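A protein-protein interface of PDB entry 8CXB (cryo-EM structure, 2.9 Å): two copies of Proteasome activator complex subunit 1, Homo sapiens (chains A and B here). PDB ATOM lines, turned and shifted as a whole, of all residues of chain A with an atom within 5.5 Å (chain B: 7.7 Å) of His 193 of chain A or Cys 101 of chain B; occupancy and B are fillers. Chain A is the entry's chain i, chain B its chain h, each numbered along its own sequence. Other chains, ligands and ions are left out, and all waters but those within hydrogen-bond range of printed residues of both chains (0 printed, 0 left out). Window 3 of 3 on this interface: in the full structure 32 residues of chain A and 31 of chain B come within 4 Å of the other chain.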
ATOM      1  N   PRO A  66      11.951 -15.773   9.514  1.00  0.00           N
ATOM      2  CA  PRO A  66      12.857 -15.961   8.389  1.00  0.00           C
ATOM      3  C   PRO A  66      13.626 -17.287   8.386  1.00  0.00           C
ATOM      4  O   PRO A  66      13.765 -17.879   9.431  1.00  0.00           O
ATOM      5  CB  PRO A  66      13.842 -14.798   8.539  1.00  0.00           C
ATOM      6  CG  PRO A  66      13.880 -14.556  10.024  1.00  0.00           C
ATOM      7  CD  PRO A  66      12.459 -14.802  10.484  1.00  0.00           C
ATOM      8  N   LYS A 190       9.331  -5.208   9.497  1.00  0.00           N
ATOM      9  CA  LYS A 190      10.468  -4.720   8.682  1.00  0.00           C
ATOM     10  C   LYS A 190      11.651  -5.649   8.885  1.00  0.00           C
ATOM     11  O   LYS A 190      12.347  -5.929   7.905  1.00  0.00           O
ATOM     12  CB  LYS A 190      10.873  -3.310   9.110  1.00  0.00           C
ATOM     13  N   GLN A 191      11.862  -6.097  10.117  1.00  0.00           N
ATOM     14  CA  GLN A 191      13.056  -6.925  10.395  1.00  0.00           C
ATOM     15  C   GLN A 191      12.615  -8.247  11.004  1.00  0.00           C
ATOM     16  O   GLN A 191      12.632  -8.371  12.234  1.00  0.00           O
ATOM     17  CB  GLN A 191      13.996  -6.180  11.334  1.00  0.00           C
ATOM     18  CG  GLN A 191      14.787  -5.078  10.648  1.00  0.00           C
ATOM     19  CD  GLN A 191      14.334  -3.705  11.073  1.00  0.00           C
ATOM     20  OE1 GLN A 191      14.976  -2.701  10.777  1.00  0.00           O
ATOM     21  NE2 GLN A 191      13.223  -3.653  11.787  1.00  0.00           N
ATOM     22  N   PRO A 192      12.242  -9.241  10.186  1.00  0.00           N
ATOM     23  CA  PRO A 192      11.767 -10.504  10.702  1.00  0.00           C
ATOM     24  C   PRO A 192      12.908 -11.165  11.470  1.00  0.00           C
ATOM     25  O   PRO A 192      12.638 -11.853  12.420  1.00  0.00           O
ATOM     26  CB  PRO A 192      11.434 -11.299   9.444  1.00  0.00           C
ATOM     27  CG  PRO A 192      11.232 -10.252   8.381  1.00  0.00           C
ATOM     28  CD  PRO A 192      12.255  -9.195   8.727  1.00  0.00           C
ATOM     29  N   HIS A 193      14.146 -10.925  11.051  1.00  0.00           N
ATOM     30  CA  HIS A 193      15.290 -11.626  11.683  1.00  0.00           C
ATOM     31  C   HIS A 193      15.335 -11.331  13.177  1.00  0.00           C
ATOM     32  O   HIS A 193      15.671 -12.243  13.932  1.00  0.00           O
ATOM     33  CB  HIS A 193      16.601 -11.280  10.977  1.00  0.00           C
ATOM     34  CG  HIS A 193      16.798  -9.831  10.703  1.00  0.00           C
ATOM     35  ND1 HIS A 193      17.519  -9.017  11.546  1.00  0.00           N
ATOM     36  CD2 HIS A 193      16.392  -9.056   9.675  1.00  0.00           C
ATOM     37  CE1 HIS A 193      17.540  -7.795  11.057  1.00  0.00           C
ATOM     38  NE2 HIS A 193      16.857  -7.793   9.910  1.00  0.00           N
ATOM     39  N   VAL A 194      15.005 -10.115  13.596  1.00  0.00           N
ATOM     40  CA  VAL A 194      15.153  -9.801  15.043  1.00  0.00           C
ATOM     41  C   VAL A 194      13.955 -10.369  15.798  1.00  0.00           C
ATOM     42  O   VAL A 194      12.833  -9.909  15.550  1.00  0.00           O
ATOM     43  CB  VAL A 194      15.310  -8.290  15.254  1.00  0.00           C
ATOM     44  CG1 VAL A 194      15.079  -7.891  16.700  1.00  0.00           C
ATOM     45  CG2 VAL A 194      16.668  -7.819  14.776  1.00  0.00           C
ATOM     46  N   GLY A 195      14.188 -11.364  16.652  1.00  0.00           N
ATOM     47  CA  GLY A 195      13.118 -11.963  17.470  1.00  0.00           C
ATOM     48  C   GLY A 195      12.636 -11.018  18.546  1.00  0.00           C
ATOM     49  O   GLY A 195      11.452 -11.093  18.907  1.00  0.00           O
ATOM     50  N   ARG A 198       9.415  -8.923  18.155  1.00  0.00           N
ATOM     51  CA  ARG A 198       8.157  -9.681  18.333  1.00  0.00           C
ATOM     52  C   ARG A 198       7.888  -9.798  19.827  1.00  0.00           C
ATOM     53  O   ARG A 198       6.731  -9.650  20.242  1.00  0.00           O
ATOM     54  CB  ARG A 198       8.270 -11.040  17.647  1.00  0.00           C
ATOM     55  CG  ARG A 198       8.373 -10.942  16.134  1.00  0.00           C
ATOM     56  CD  ARG A 198       9.644 -11.554  15.585  1.00  0.00           C
ATOM     57  NE  ARG A 198       9.501 -12.983  15.364  1.00  0.00           N
ATOM     58  CZ  ARG A 198      10.466 -13.770  14.905  1.00  0.00           C
ATOM     59  NH1 ARG A 198      11.654 -13.265  14.623  1.00  0.00           N
ATOM     60  NH2 ARG A 198      10.242 -15.059  14.733  1.00  0.00           N
ATOM     61  N   ASP B  62      23.970 -15.014  15.649  1.00  0.00           N
ATOM     62  CA  ASP B  62      24.219 -15.789  14.407  1.00  0.00           C
ATOM     63  C   ASP B  62      24.558 -14.856  13.251  1.00  0.00           C
ATOM     64  O   ASP B  62      24.727 -15.358  12.130  1.00  0.00           O
ATOM     65  CB  ASP B  62      22.980 -16.599  14.032  1.00  0.00           C
ATOM     66  N   ILE B  63      24.634 -13.553  13.501  1.00  0.00           N
ATOM     67  CA  ILE B  63      24.847 -12.614  12.367  1.00  0.00           C
ATOM     68  C   ILE B  63      26.173 -12.975  11.702  1.00  0.00           C
ATOM     69  O   ILE B  63      27.156 -13.214  12.419  1.00  0.00           O
ATOM     70  CB  ILE B  63      24.800 -11.161  12.869  1.00  0.00           C
ATOM     71  CG1 ILE B  63      25.316 -10.173  11.823  1.00  0.00           C
ATOM     72  CG2 ILE B  63      25.542 -11.020  14.188  1.00  0.00           C
ATOM     73  CD1 ILE B  63      25.989  -8.970  12.420  1.00  0.00           C
ATOM     74  N   PRO B  64      26.225 -13.055  10.357  1.00  0.00           N
ATOM     75  CA  PRO B  64      27.455 -13.386   9.646  1.00  0.00           C
ATOM     76  C   PRO B  64      28.528 -12.303   9.810  1.00  0.00           C
ATOM     77  O   PRO B  64      28.180 -11.148   9.845  1.00  0.00           O
ATOM     78  CB  PRO B  64      27.011 -13.428   8.180  1.00  0.00           C
ATOM     79  CG  PRO B  64      25.759 -12.589   8.132  1.00  0.00           C
ATOM     80  CD  PRO B  64      25.088 -12.864   9.457  1.00  0.00           C
ATOM     81  N   PRO B 100      20.206 -11.284   5.287  1.00  0.00           N
ATOM     82  CA  PRO B 100      20.351 -12.736   5.152  1.00  0.00           C
ATOM     83  C   PRO B 100      20.584 -13.389   6.519  1.00  0.00           C
ATOM     84  O   PRO B 100      20.814 -14.581   6.565  1.00  0.00           O
ATOM     85  CB  PRO B 100      21.611 -12.907   4.292  1.00  0.00           C
ATOM     86  CG  PRO B 100      22.452 -11.716   4.660  1.00  0.00           C
ATOM     87  CD  PRO B 100      21.443 -10.607   4.873  1.00  0.00           C
ATOM     88  N   CYS B 101      20.529 -12.594   7.588  1.00  0.00           N
ATOM     89  CA  CYS B 101      20.686 -13.167   8.947  1.00  0.00           C
ATOM     90  C   CYS B 101      19.482 -14.055   9.254  1.00  0.00           C
ATOM     91  O   CYS B 101      18.355 -13.657   8.918  1.00  0.00           O
ATOM     92  CB  CYS B 101      20.811 -12.071   9.995  1.00  0.00           C
ATOM     93  N   GLY B 102      19.718 -15.219   9.853  1.00  0.00           N
ATOM     94  CA  GLY B 102      18.608 -16.090  10.274  1.00  0.00           C
ATOM     95  C   GLY B 102      17.989 -15.515  11.521  1.00  0.00           C
ATOM     96  O   GLY B 102      18.621 -14.638  12.121  1.00  0.00           O
ATOM     97  N   PRO B 103      16.804 -15.961  11.969  1.00  0.00           N
ATOM     98  CA  PRO B 103      16.175 -15.317  13.100  1.00  0.00           C
ATOM     99  C   PRO B 103      17.193 -15.365  14.238  1.00  0.00           C
ATOM    100  O   PRO B 103      17.715 -16.419  14.524  1.00  0.00           O
ATOM    101  CB  PRO B 103      14.968 -16.201  13.422  1.00  0.00           C
ATOM    102  CG  PRO B 103      15.200 -17.484  12.647  1.00  0.00           C
ATOM    103  CD  PRO B 103      16.063 -17.106  11.462  1.00  0.00           C
ATOM    104  N   VAL B 104      17.434 -14.215  14.859  1.00  0.00           N
ATOM    105  CA  VAL B 104      18.402 -14.167  15.985  1.00  0.00           C
ATOM    106  C   VAL B 104      17.578 -14.231  17.263  1.00  0.00           C
ATOM    107  O   VAL B 104      16.701 -13.376  17.456  1.00  0.00           O
ATOM    108  CB  VAL B 104      19.315 -12.935  15.898  1.00  0.00           C
ATOM    109  CG1 VAL B 104      20.453 -13.165  14.916  1.00  0.00           C
ATOM    110  CG2 VAL B 104      18.551 -11.673  15.531  1.00  0.00           C
ATOM    111  N   ASN B 105      17.818 -15.250  18.077  1.00  0.00           N
ATOM    112  CA  ASN B 105      16.972 -15.449  19.273  1.00  0.00           C
ATOM    113  C   ASN B 105      17.397 -14.508  20.394  1.00  0.00           C
ATOM    114  O   ASN B 105      18.502 -13.955  20.305  1.00  0.00           O
ATOM    115  CB  ASN B 105      16.997 -16.912  19.694  1.00  0.00           C
ATOM    116  CG  ASN B 105      16.467 -17.823  18.609  1.00  0.00           C
ATOM    117  OD1 ASN B 105      16.096 -17.362  17.532  1.00  0.00           O
ATOM    118  ND2 ASN B 105      16.424 -19.116  18.884  1.00  0.00           N
ATOM    119  N   GLY B 182      16.474  -4.988  20.872  1.00  0.00           N
ATOM    120  CA  GLY B 182      15.997  -5.220  19.504  1.00  0.00           C
ATOM    121  C   GLY B 182      16.657  -4.266  18.547  1.00  0.00           C
ATOM    122  O   GLY B 182      17.019  -4.684  17.444  1.00  0.00           O
ATOM    123  N   VAL B 185      20.257  -5.465  18.060  1.00  0.00           N
ATOM    124  CA  VAL B 185      20.469  -6.588  17.114  1.00  0.00           C
ATOM    125  C   VAL B 185      20.232  -6.080  15.693  1.00  0.00           C
ATOM    126  O   VAL B 185      20.998  -6.472  14.812  1.00  0.00           O
ATOM    127  CB  VAL B 185      19.669  -7.857  17.450  1.00  0.00           C
ATOM    128  CG1 VAL B 185      20.458  -8.810  18.326  1.00  0.00           C
ATOM    129  CG2 VAL B 185      18.326  -7.558  18.075  1.00  0.00           C
ATOM    130  N   THR B 186      19.221  -5.240  15.471  1.00  0.00           N
ATOM    131  CA  THR B 186      18.980  -4.828  14.069  1.00  0.00           C
ATOM    132  C   THR B 186      20.199  -4.072  13.576  1.00  0.00           C
ATOM    133  O   THR B 186      20.600  -4.282  12.429  1.00  0.00           O
ATOM    134  CB  THR B 186      17.871  -3.793  13.921  1.00  0.00           C
ATOM    135  OG1 THR B 186      17.976  -2.797  14.935  1.00  0.00           O
ATOM    136  CG2 THR B 186      16.493  -4.406  13.943  1.00  0.00           C
ATOM    137  N   LYS B 187      20.747  -3.212  14.426  1.00  0.00           N
ATOM    138  CA  LYS B 187      21.892  -2.399  13.977  1.00  0.00           C
ATOM    139  C   LYS B 187      22.995  -3.386  13.646  1.00  0.00           C
ATOM    140  O   LYS B 187      23.633  -3.230  12.604  1.00  0.00           O
ATOM    141  CB  LYS B 187      22.353  -1.457  15.085  1.00  0.00           C
ATOM    142  CG  LYS B 187      21.542  -0.179  15.230  1.00  0.00           C
ATOM    143  CD  LYS B 187      21.980   0.647  16.412  1.00  0.00           C
ATOM    144  CE  LYS B 187      21.328   2.011  16.453  1.00  0.00           C
ATOM    145  NZ  LYS B 187      21.805   2.801  17.611  1.00  0.00           N
ATOM    146  N   ALA B 188      23.168  -4.392  14.488  1.00  0.00           N
ATOM    147  CA  ALA B 188      24.285  -5.311  14.234  1.00  0.00           C
ATOM    148  C   ALA B 188      24.033  -5.975  12.891  1.00  0.00           C
ATOM    149  O   ALA B 188      24.946  -6.000  12.062  1.00  0.00           O
ATOM    150  CB  ALA B 188      24.333  -6.340  15.316  1.00  0.00           C
ATOM    151  N   ALA B 189      22.807  -6.429  12.665  1.00  0.00           N
ATOM    152  CA  ALA B 189      22.522  -7.154  11.414  1.00  0.00           C
ATOM    153  C   ALA B 189      22.724  -6.223  10.222  1.00  0.00           C
ATOM    154  O   ALA B 189      23.370  -6.645   9.254  1.00  0.00           O
ATOM    155  CB  ALA B 189      21.111  -7.658  11.452  1.00  0.00           C
ATOM    156  N   LYS B 190      22.225  -4.992  10.306  1.00  0.00           N
ATOM    157  CA  LYS B 190      22.305  -4.069   9.148  1.00  0.00           C
ATOM    158  C   LYS B 190      23.774  -3.791   8.854  1.00  0.00           C
ATOM    159  O   LYS B 190      24.129  -3.696   7.673  1.00  0.00           O
ATOM    160  CB  LYS B 190      21.528  -2.779   9.410  1.00  0.00           C
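N of Val 104 of chain B is in hydrogen-bond range of O of His 193 of chain A, at 2.8 Å. The backbone carbonyl oxygen (O) of Val 104 of chain B is in hydrogen-bond range of the backbone NH (N) of Gly 195 of chain A (3.3 Å).
The backbone carbonyl oxygen (O) of Gly 182 of chain B sits at hydrogen-bond distance from the side-chain hydroxyl (OG1) of Thr 186 of chain B.
1 position is printed for both chains. Of the 11 pairs that touch across the chains among the printed residues, none has its exchanged pair printed and touching as well.
Of the 16 printed residues of chain B, 7 touch a printed residue of chain A. Hydrophobic or aromatic side chains of chain B within 4 Å of the printed part of chain A: Pro 103, Val 104, Val 185 and Ala 189. Among the printed residues, 11 pairs touch across the chains. Among the printed residues, no Asp or Glu carboxylate lies within 4 Å of a Lys or Arg side-chain nitrogen of the other chain.
Among the printed residues, pairs that only touch across the chains: Pro 66 of chain A with Pro 103 of chain B, His 193 of chain A with Pro 103 of chain B, Val 194 of chain A with Thr 186 of chain B, Val 194 of chain A with Val 185 of chain B, His 193 of chain A with Ala 189 of chain B, His 193 of chain A with Cys 101 of chain B, Gln 191 of chain A with Thr 186 of chain B, Val 194 of chain A with Gly 182 of chain B and Val 194 of chain A with Val 104 of chain B.
Printed residues of chain A within 4 Å of Cys 101 of chain B: His 193. Printed residues of chain A within 4 Å of Gly 182 of chain B: Val 194 (3.8 Å). Of the printed residues of chain A, Val 185 of chain B touches Val 194 (3.5 Å). Ala 188 of chain B touches none of the printed residues of chain A. The nearest residue of chain B that does not touch His 193 of chain A is Gly 102 of chain B (4.1 Å). The nearest residue of chain A that does not touch Cys 101 of chain B is Pro 66 of chain A (4.7 Å). The nearest printed residue of chain A that does not touch Thr 186 of chain B is His 193 of chain A (4.5 Å).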
